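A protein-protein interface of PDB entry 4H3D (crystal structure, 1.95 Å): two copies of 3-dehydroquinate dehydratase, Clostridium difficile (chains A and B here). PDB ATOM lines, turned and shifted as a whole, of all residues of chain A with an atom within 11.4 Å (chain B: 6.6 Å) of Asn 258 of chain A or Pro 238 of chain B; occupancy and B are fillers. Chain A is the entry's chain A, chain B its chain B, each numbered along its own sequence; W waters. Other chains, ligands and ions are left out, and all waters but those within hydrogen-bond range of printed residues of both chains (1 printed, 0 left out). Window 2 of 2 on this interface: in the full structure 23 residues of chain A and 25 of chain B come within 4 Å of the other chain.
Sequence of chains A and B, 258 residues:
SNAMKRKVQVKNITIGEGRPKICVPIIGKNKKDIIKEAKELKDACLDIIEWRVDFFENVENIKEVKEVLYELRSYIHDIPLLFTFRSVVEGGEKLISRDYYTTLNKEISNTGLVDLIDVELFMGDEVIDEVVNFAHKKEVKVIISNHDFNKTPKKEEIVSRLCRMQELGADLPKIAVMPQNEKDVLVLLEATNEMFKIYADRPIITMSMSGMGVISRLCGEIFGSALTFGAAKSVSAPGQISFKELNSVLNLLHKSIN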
ATOM      1  N   GLU A 221     -24.085  15.752  -6.139  1.00  0.00           N
ATOM      2  CA  GLU A 221     -25.480  16.030  -5.948  1.00  0.00           C
ATOM      3  C   GLU A 221     -25.738  17.536  -6.075  1.00  0.00           C
ATOM      4  O   GLU A 221     -26.709  17.938  -6.673  1.00  0.00           O
ATOM      5  CB  GLU A 221     -25.988  15.483  -4.615  1.00  0.00           C
ATOM      6  CG  GLU A 221     -27.497  15.597  -4.457  1.00  0.00           C
ATOM      7  CD  GLU A 221     -28.036  14.784  -3.296  1.00  0.00           C
ATOM      8  OE1 GLU A 221     -29.255  14.841  -3.060  1.00  0.00           O
ATOM      9  OE2 GLU A 221     -27.246  14.071  -2.631  1.00  0.00           O
ATOM     10  N   ILE A 222     -24.841  18.352  -5.535  1.00  0.00           N
ATOM     11  CA  ILE A 222     -24.985  19.799  -5.648  1.00  0.00           C
ATOM     12  C   ILE A 222     -24.670  20.316  -7.049  1.00  0.00           C
ATOM     13  O   ILE A 222     -25.420  21.107  -7.593  1.00  0.00           O
ATOM     14  CB  ILE A 222     -24.101  20.552  -4.637  1.00  0.00           C
ATOM     15  CG1 ILE A 222     -24.572  20.273  -3.200  1.00  0.00           C
ATOM     16  CG2 ILE A 222     -24.162  22.098  -4.896  1.00  0.00           C
ATOM     17  CD1 ILE A 222     -26.043  20.732  -2.950  1.00  0.00           C
ATOM     18  N   ASN A 251     -24.094  10.061   1.421  1.00  0.00           N
ATOM     19  CA  ASN A 251     -25.340  10.108   2.209  1.00  0.00           C
ATOM     20  C   ASN A 251     -25.323  11.254   3.188  1.00  0.00           C
ATOM     21  O   ASN A 251     -26.337  11.915   3.390  1.00  0.00           O
ATOM     22  CB  ASN A 251     -25.642   8.764   2.859  1.00  0.00           C
ATOM     23  CG  ASN A 251     -26.337   7.801   1.880  1.00  0.00           C
ATOM     24  OD1 ASN A 251     -27.444   8.091   1.395  1.00  0.00           O
ATOM     25  ND2 ASN A 251     -25.695   6.675   1.586  1.00  0.00           N
ATOM     26  N   LEU A 252     -24.150  11.512   3.753  1.00  0.00           N
ATOM     27  CA  LEU A 252     -23.934  12.644   4.649  1.00  0.00           C
ATOM     28  C   LEU A 252     -24.303  13.941   3.925  1.00  0.00           C
ATOM     29  O   LEU A 252     -25.005  14.786   4.467  1.00  0.00           O
ATOM     30  CB  LEU A 252     -22.459  12.677   5.071  1.00  0.00           C
ATOM     31  CG  LEU A 252     -21.911  13.804   5.937  1.00  0.00           C
ATOM     32  CD1 LEU A 252     -20.415  13.602   6.085  1.00  0.00           C
ATOM     33  CD2 LEU A 252     -22.181  15.160   5.355  1.00  0.00           C
ATOM     34  N   LEU A 253     -23.830  14.086   2.689  1.00  0.00           N
ATOM     35  CA  LEU A 253     -24.102  15.288   1.905  1.00  0.00           C
ATOM     36  C   LEU A 253     -25.553  15.345   1.401  1.00  0.00           C
ATOM     37  O   LEU A 253     -26.136  16.427   1.272  1.00  0.00           O
ATOM     38  CB  LEU A 253     -23.106  15.411   0.749  1.00  0.00           C
ATOM     39  CG  LEU A 253     -21.639  15.531   1.188  1.00  0.00           C
ATOM     40  CD1 LEU A 253     -20.706  15.663  -0.044  1.00  0.00           C
ATOM     41  CD2 LEU A 253     -21.441  16.694   2.127  1.00  0.00           C
ATOM     42  N   HIS A 254     -26.135  14.188   1.126  1.00  0.00           N
ATOM     43  CA  HIS A 254     -27.528  14.133   0.698  1.00  0.00           C
ATOM     44  C   HIS A 254     -28.455  14.651   1.825  1.00  0.00           C
ATOM     45  O   HIS A 254     -29.451  15.325   1.551  1.00  0.00           O
ATOM     46  CB  HIS A 254     -27.904  12.714   0.275  1.00  0.00           C
ATOM     47  CG  HIS A 254     -29.347  12.549  -0.085  1.00  0.00           C
ATOM     48  ND1 HIS A 254     -29.879  13.018  -1.266  1.00  0.00           N
ATOM     49  CD2 HIS A 254     -30.367  11.950   0.575  1.00  0.00           C
ATOM     50  CE1 HIS A 254     -31.167  12.724  -1.315  1.00  0.00           C
ATOM     51  NE2 HIS A 254     -31.487  12.075  -0.210  1.00  0.00           N
ATOM     52  N   LYS A 255     -28.107  14.361   3.077  1.00  0.00           N
ATOM     53  CA  LYS A 255     -28.914  14.827   4.221  1.00  0.00           C
ATOM     54  C   LYS A 255     -28.708  16.309   4.539  1.00  0.00           C
ATOM     55  O   LYS A 255     -29.586  16.944   5.099  1.00  0.00           O
ATOM     56  CB  LYS A 255     -28.613  14.003   5.478  1.00  0.00           C
ATOM     57  CG  LYS A 255     -29.076  12.554   5.411  1.00  0.00           C
ATOM     58  CD  LYS A 255     -28.835  11.852   6.745  1.00  0.00           C
ATOM     59  CE  LYS A 255     -29.328  10.410   6.723  1.00  0.00           C
ATOM     60  NZ  LYS A 255     -29.166   9.762   8.054  1.00  0.00           N
ATOM     61  N   SER A 256     -27.554  16.858   4.170  1.00  0.00           N
ATOM     62  CA  SER A 256     -27.247  18.247   4.471  1.00  0.00           C
ATOM     63  C   SER A 256     -27.865  19.251   3.491  1.00  0.00           C
ATOM     64  O   SER A 256     -27.658  20.447   3.648  1.00  0.00           O
ATOM     65  CB  SER A 256     -25.730  18.466   4.493  1.00  0.00           C
ATOM     66  OG  SER A 256     -25.190  18.481   3.175  1.00  0.00           O
ATOM     67  N   ILE A 257     -28.603  18.773   2.481  1.00  0.00           N
ATOM     68  CA  ILE A 257     -29.211  19.680   1.482  1.00  0.00           C
ATOM     69  C   ILE A 257     -30.393  20.433   2.071  1.00  0.00           C
ATOM     70  O   ILE A 257     -31.067  19.931   2.979  1.00  0.00           O
ATOM     71  CB  ILE A 257     -29.674  18.934   0.189  1.00  0.00           C
ATOM     72  CG1 ILE A 257     -30.810  17.938   0.506  1.00  0.00           C
ATOM     73  CG2 ILE A 257     -28.486  18.257  -0.498  1.00  0.00           C
ATOM     74  CD1 ILE A 257     -31.168  17.004  -0.657  1.00  0.00           C
ATOM     75  N   ASN A 258     -30.641  21.639   1.553  1.00  0.00           N
ATOM     76  CA  ASN A 258     -31.758  22.477   2.009  1.00  0.00           C
ATOM     77  C   ASN A 258     -33.108  22.009   1.454  1.00  0.00           C
ATOM     78  O   ASN A 258     -34.108  22.731   1.546  1.00  0.00           O
ATOM     79  CB  ASN A 258     -31.522  23.927   1.596  1.00  0.00           C
ATOM     80  CG  ASN A 258     -30.299  24.526   2.250  1.00  0.00           C
ATOM     81  OD1 ASN A 258     -29.343  24.880   1.574  1.00  0.00           O
ATOM     82  ND2 ASN A 258     -30.311  24.611   3.578  1.00  0.00           N
ATOM     83  OXT ASN A 258     -33.242  20.910   0.900  1.00  0.00           O
ATOM     84  N   MET B 209     -22.326  29.257   3.222  1.00  0.00           N
ATOM     85  CA  MET B 209     -23.329  28.669   4.088  1.00  0.00           C
ATOM     86  C   MET B 209     -24.425  27.921   3.297  1.00  0.00           C
ATOM     87  O   MET B 209     -24.383  27.877   2.073  1.00  0.00           O
ATOM     88  CB  MET B 209     -23.939  29.773   4.965  1.00  0.00           C
ATOM     89  CG  MET B 209     -22.911  30.453   5.894  1.00  0.00           C
ATOM     90  SD  MET B 209     -23.632  31.740   6.961  1.00  0.00           S
ATOM     91  CE  MET B 209     -24.056  32.983   5.758  1.00  0.00           C
ATOM     92  N   SER B 210     -25.366  27.306   4.038  1.00  0.00           N
ATOM     93  CA  SER B 210     -26.483  26.505   3.500  1.00  0.00           C
ATOM     94  C   SER B 210     -26.003  25.138   2.965  1.00  0.00           C
ATOM     95  O   SER B 210     -24.800  24.899   2.846  1.00  0.00           O
ATOM     96  CB  SER B 210     -27.256  27.239   2.405  1.00  0.00           C
ATOM     97  OG  SER B 210     -26.613  27.136   1.147  1.00  0.00           O
ATOM     98  N   GLY B 211     -26.964  24.270   2.618  1.00  0.00           N
ATOM     99  CA  GLY B 211     -26.673  22.913   2.083  1.00  0.00           C
ATOM    100  C   GLY B 211     -25.823  22.973   0.837  1.00  0.00           C
ATOM    101  O   GLY B 211     -24.894  22.200   0.658  1.00  0.00           O
ATOM    102  N   MET B 212     -26.141  23.929  -0.015  1.00  0.00           N
ATOM    103  CA  MET B 212     -25.431  24.157  -1.259  1.00  0.00           C
ATOM    104  C   MET B 212     -23.942  24.486  -1.039  1.00  0.00           C
ATOM    105  O   MET B 212     -23.100  24.145  -1.869  1.00  0.00           O
ATOM    106  CB  MET B 212     -26.136  25.321  -1.988  1.00  0.00           C
ATOM    107  CG  MET B 212     -25.652  25.662  -3.360  1.00  0.00           C
ATOM    108  SD  MET B 212     -26.717  26.931  -4.136  1.00  0.00           S
ATOM    109  CE  MET B 212     -28.235  26.016  -4.323  1.00  0.00           C
ATOM    110  N   GLY B 213     -23.615  25.133   0.087  1.00  0.00           N
ATOM    111  CA  GLY B 213     -22.244  25.567   0.337  1.00  0.00           C
ATOM    112  C   GLY B 213     -21.343  24.622   1.117  1.00  0.00           C
ATOM    113  O   GLY B 213     -20.186  24.946   1.351  1.00  0.00           O
ATOM    114  N   VAL B 214     -21.854  23.449   1.475  1.00  0.00           N
ATOM    115  CA  VAL B 214     -21.111  22.490   2.330  1.00  0.00           C
ATOM    116  C   VAL B 214     -19.722  22.108   1.817  1.00  0.00           C
ATOM    117  O   VAL B 214     -18.810  21.905   2.619  1.00  0.00           O
ATOM    118  CB  VAL B 214     -21.939  21.231   2.602  1.00  0.00           C
ATOM    119  CG1 VAL B 214     -21.109  20.185   3.349  1.00  0.00           C
ATOM    120  CG2 VAL B 214     -23.189  21.602   3.396  1.00  0.00           C
ATOM    121  N   VAL B 235     -27.279  16.208  14.075  1.00  0.00           N
ATOM    122  CA  VAL B 235     -28.447  16.694  13.329  1.00  0.00           C
ATOM    123  C   VAL B 235     -28.081  18.021  12.632  1.00  0.00           C
ATOM    124  O   VAL B 235     -27.523  18.933  13.259  1.00  0.00           O
ATOM    125  CB  VAL B 235     -29.687  16.885  14.251  1.00  0.00           C
ATOM    126  CG1 VAL B 235     -30.239  15.535  14.698  1.00  0.00           C
ATOM    127  CG2 VAL B 235     -29.340  17.762  15.456  1.00  0.00           C
ATOM    128  N   SER B 236     -28.391  18.116  11.338  1.00  0.00           N
ATOM    129  CA  SER B 236     -28.059  19.310  10.543  1.00  0.00           C
ATOM    130  C   SER B 236     -29.027  20.474  10.813  1.00  0.00           C
ATOM    131  O   SER B 236     -30.037  20.309  11.501  1.00  0.00           O
ATOM    132  CB  SER B 236     -28.049  18.967   9.039  1.00  0.00           C
ATOM    133  OG  SER B 236     -29.360  18.691   8.549  1.00  0.00           O
ATOM    134  N   ALA B 237     -28.697  21.650  10.272  1.00  0.00           N
ATOM    135  CA  ALA B 237     -29.529  22.851  10.430  1.00  0.00           C
ATOM    136  C   ALA B 237     -30.702  22.963   9.424  1.00  0.00           C
ATOM    137  O   ALA B 237     -31.780  23.445   9.799  1.00  0.00           O
ATOM    138  CB  ALA B 237     -28.663  24.111  10.376  1.00  0.00           C
ATOM    139  N   PRO B 238     -30.521  22.510   8.154  1.00  0.00           N
ATOM    140  CA  PRO B 238     -29.379  21.874   7.475  1.00  0.00           C
ATOM    141  C   PRO B 238     -28.248  22.841   7.101  1.00  0.00           C
ATOM    142  O   PRO B 238     -28.263  23.998   7.505  1.00  0.00           O
ATOM    143  CB  PRO B 238     -30.018  21.272   6.222  1.00  0.00           C
ATOM    144  CG  PRO B 238     -31.139  22.168   5.921  1.00  0.00           C
ATOM    145  CD  PRO B 238     -31.673  22.641   7.240  1.00  0.00           C
ATOM    146  N   GLY B 239     -27.283  22.357   6.326  1.00  0.00           N
ATOM    147  CA  GLY B 239     -26.124  23.156   5.954  1.00  0.00           C
ATOM    148  C   GLY B 239     -24.986  22.989   6.968  1.00  0.00           C
ATOM    149  O   GLY B 239     -23.971  23.692   6.894  1.00  0.00           O
ATOM    150  N   GLN B 240     -25.170  22.063   7.913  1.00  0.00           N
ATOM    151  CA  GLN B 240     -24.176  21.774   8.955  1.00  0.00           C
ATOM    152  C   GLN B 240     -23.725  20.316   8.843  1.00  0.00           C
ATOM    153  O   GLN B 240     -24.452  19.472   8.331  1.00  0.00           O
ATOM    154  CB  GLN B 240     -24.779  21.996  10.342  1.00  0.00           C
ATOM    155  CG  GLN B 240     -25.277  23.422  10.625  1.00  0.00           C
ATOM    156  CD  GLN B 240     -24.160  24.436  10.868  1.00  0.00           C
ATOM    157  OE1 GLN B 240     -22.995  24.078  11.080  1.00  0.00           O
ATOM    158  NE2 GLN B 240     -24.524  25.714  10.856  1.00  0.00           N
HETATM  159  O   HOH W   1     -24.785  19.485   0.672  1.00  0.00           O
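O of Ser 256 of chain A is in hydrogen-bond range of N of Gly 239 of chain B, 3.3 Å away.
N of Gly 211 of chain B is in hydrogen-bond range of OD1 of Asn 258 of chain A (2.7 Å).
O of Leu 253 of chain A sits at hydrogen-bond distance from OG of Ser 256 of chain A, at 3.0 Å.
OG of Ser 210 of chain B lies close to N of Met 212 of chain B (3.4 Å).
CG2 of Ile 222 of chain A touches O of Met 212 of chain B (3.8 Å).
Val 214 of chain B touches Leu 253 of chain A (CG1 to CD2, 3.7 Å).
Ser 236 of chain B touches Lys 255 of chain A (OG to O, 3.9 Å).
Ser 256 of chain A touches Gly 211 of chain B (O to CA, 3.1 Å).
Val 214 of chain B touches Ser 256 of chain A (CG2 to OG, 3.7 Å).
Pro 238 of chain B touches Ser 256 of chain A (CB to O, 3.6 Å).
O of Ile 257 of chain A touches CB of Pro 238 of chain B (3.7 Å).
CB of Ser 210 of chain B touches OD1 of Asn 258 of chain A, at 3.3 Å.
Asn 258 of chain A touches Met 212 of chain B (OD1 to N, 3.7 Å).
Pro 238 of chain B touches Asn 258 of chain A (CG to ND2, 3.5 Å).
Of the printed residues of chain B, Ile 222 of chain A touches Met 212.
Of the printed residues of chain B, Leu 253 of chain A touches Val 214.
Of the printed residues of chain B, Lys 255 of chain A touches Ser 236.
Printed residues of chain B within 4 Å of Ile 257 of chain A: Pro 238.
Asn 258 of chain A touches just these residues of chain B: Ser 210, Gly 211, Met 212 and Pro 238.
Ser 210 of chain B touches one residue of chain A.
Gly 211 of chain B touches two residues of chain A.
Of the printed residues of chain A, Val 214 of chain B touches Leu 253 and Ser 256.
No residue of chain A comes within 4 Å of Ala 237 of chain B.
Pro 238 of chain B touches just these residues of chain A: Ser 256 (3.6 Å), Ile 257 (3.7 Å) and Asn 258 (3.5 Å).
Of the printed residues of chain A, Gly 239 of chain B touches Ser 256 (3.3 Å).
The nearest printed residue of chain B that does not touch Lys 255 of chain A is Pro 238 of chain B (4.5 Å).
Of the 10 printed residues of chain A, 6 touch a printed residue of chain B.
Hydrophobic or aromatic side chains of chain B that line the printed part of chain A: Val 214 and Pro 238.
Among the printed residues, no Asp or Glu carboxylate lies within 4 Å of a Lys or Arg side-chain nitrogen of the other chain.
No position is printed for both chains.
Water W1 lies within hydrogen-bond range of O of Gly 211 of chain B (2.7 Å), OG of Ser 256 of chain A (2.7 Å) and O of Leu 253 of chain A (3.4 Å).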
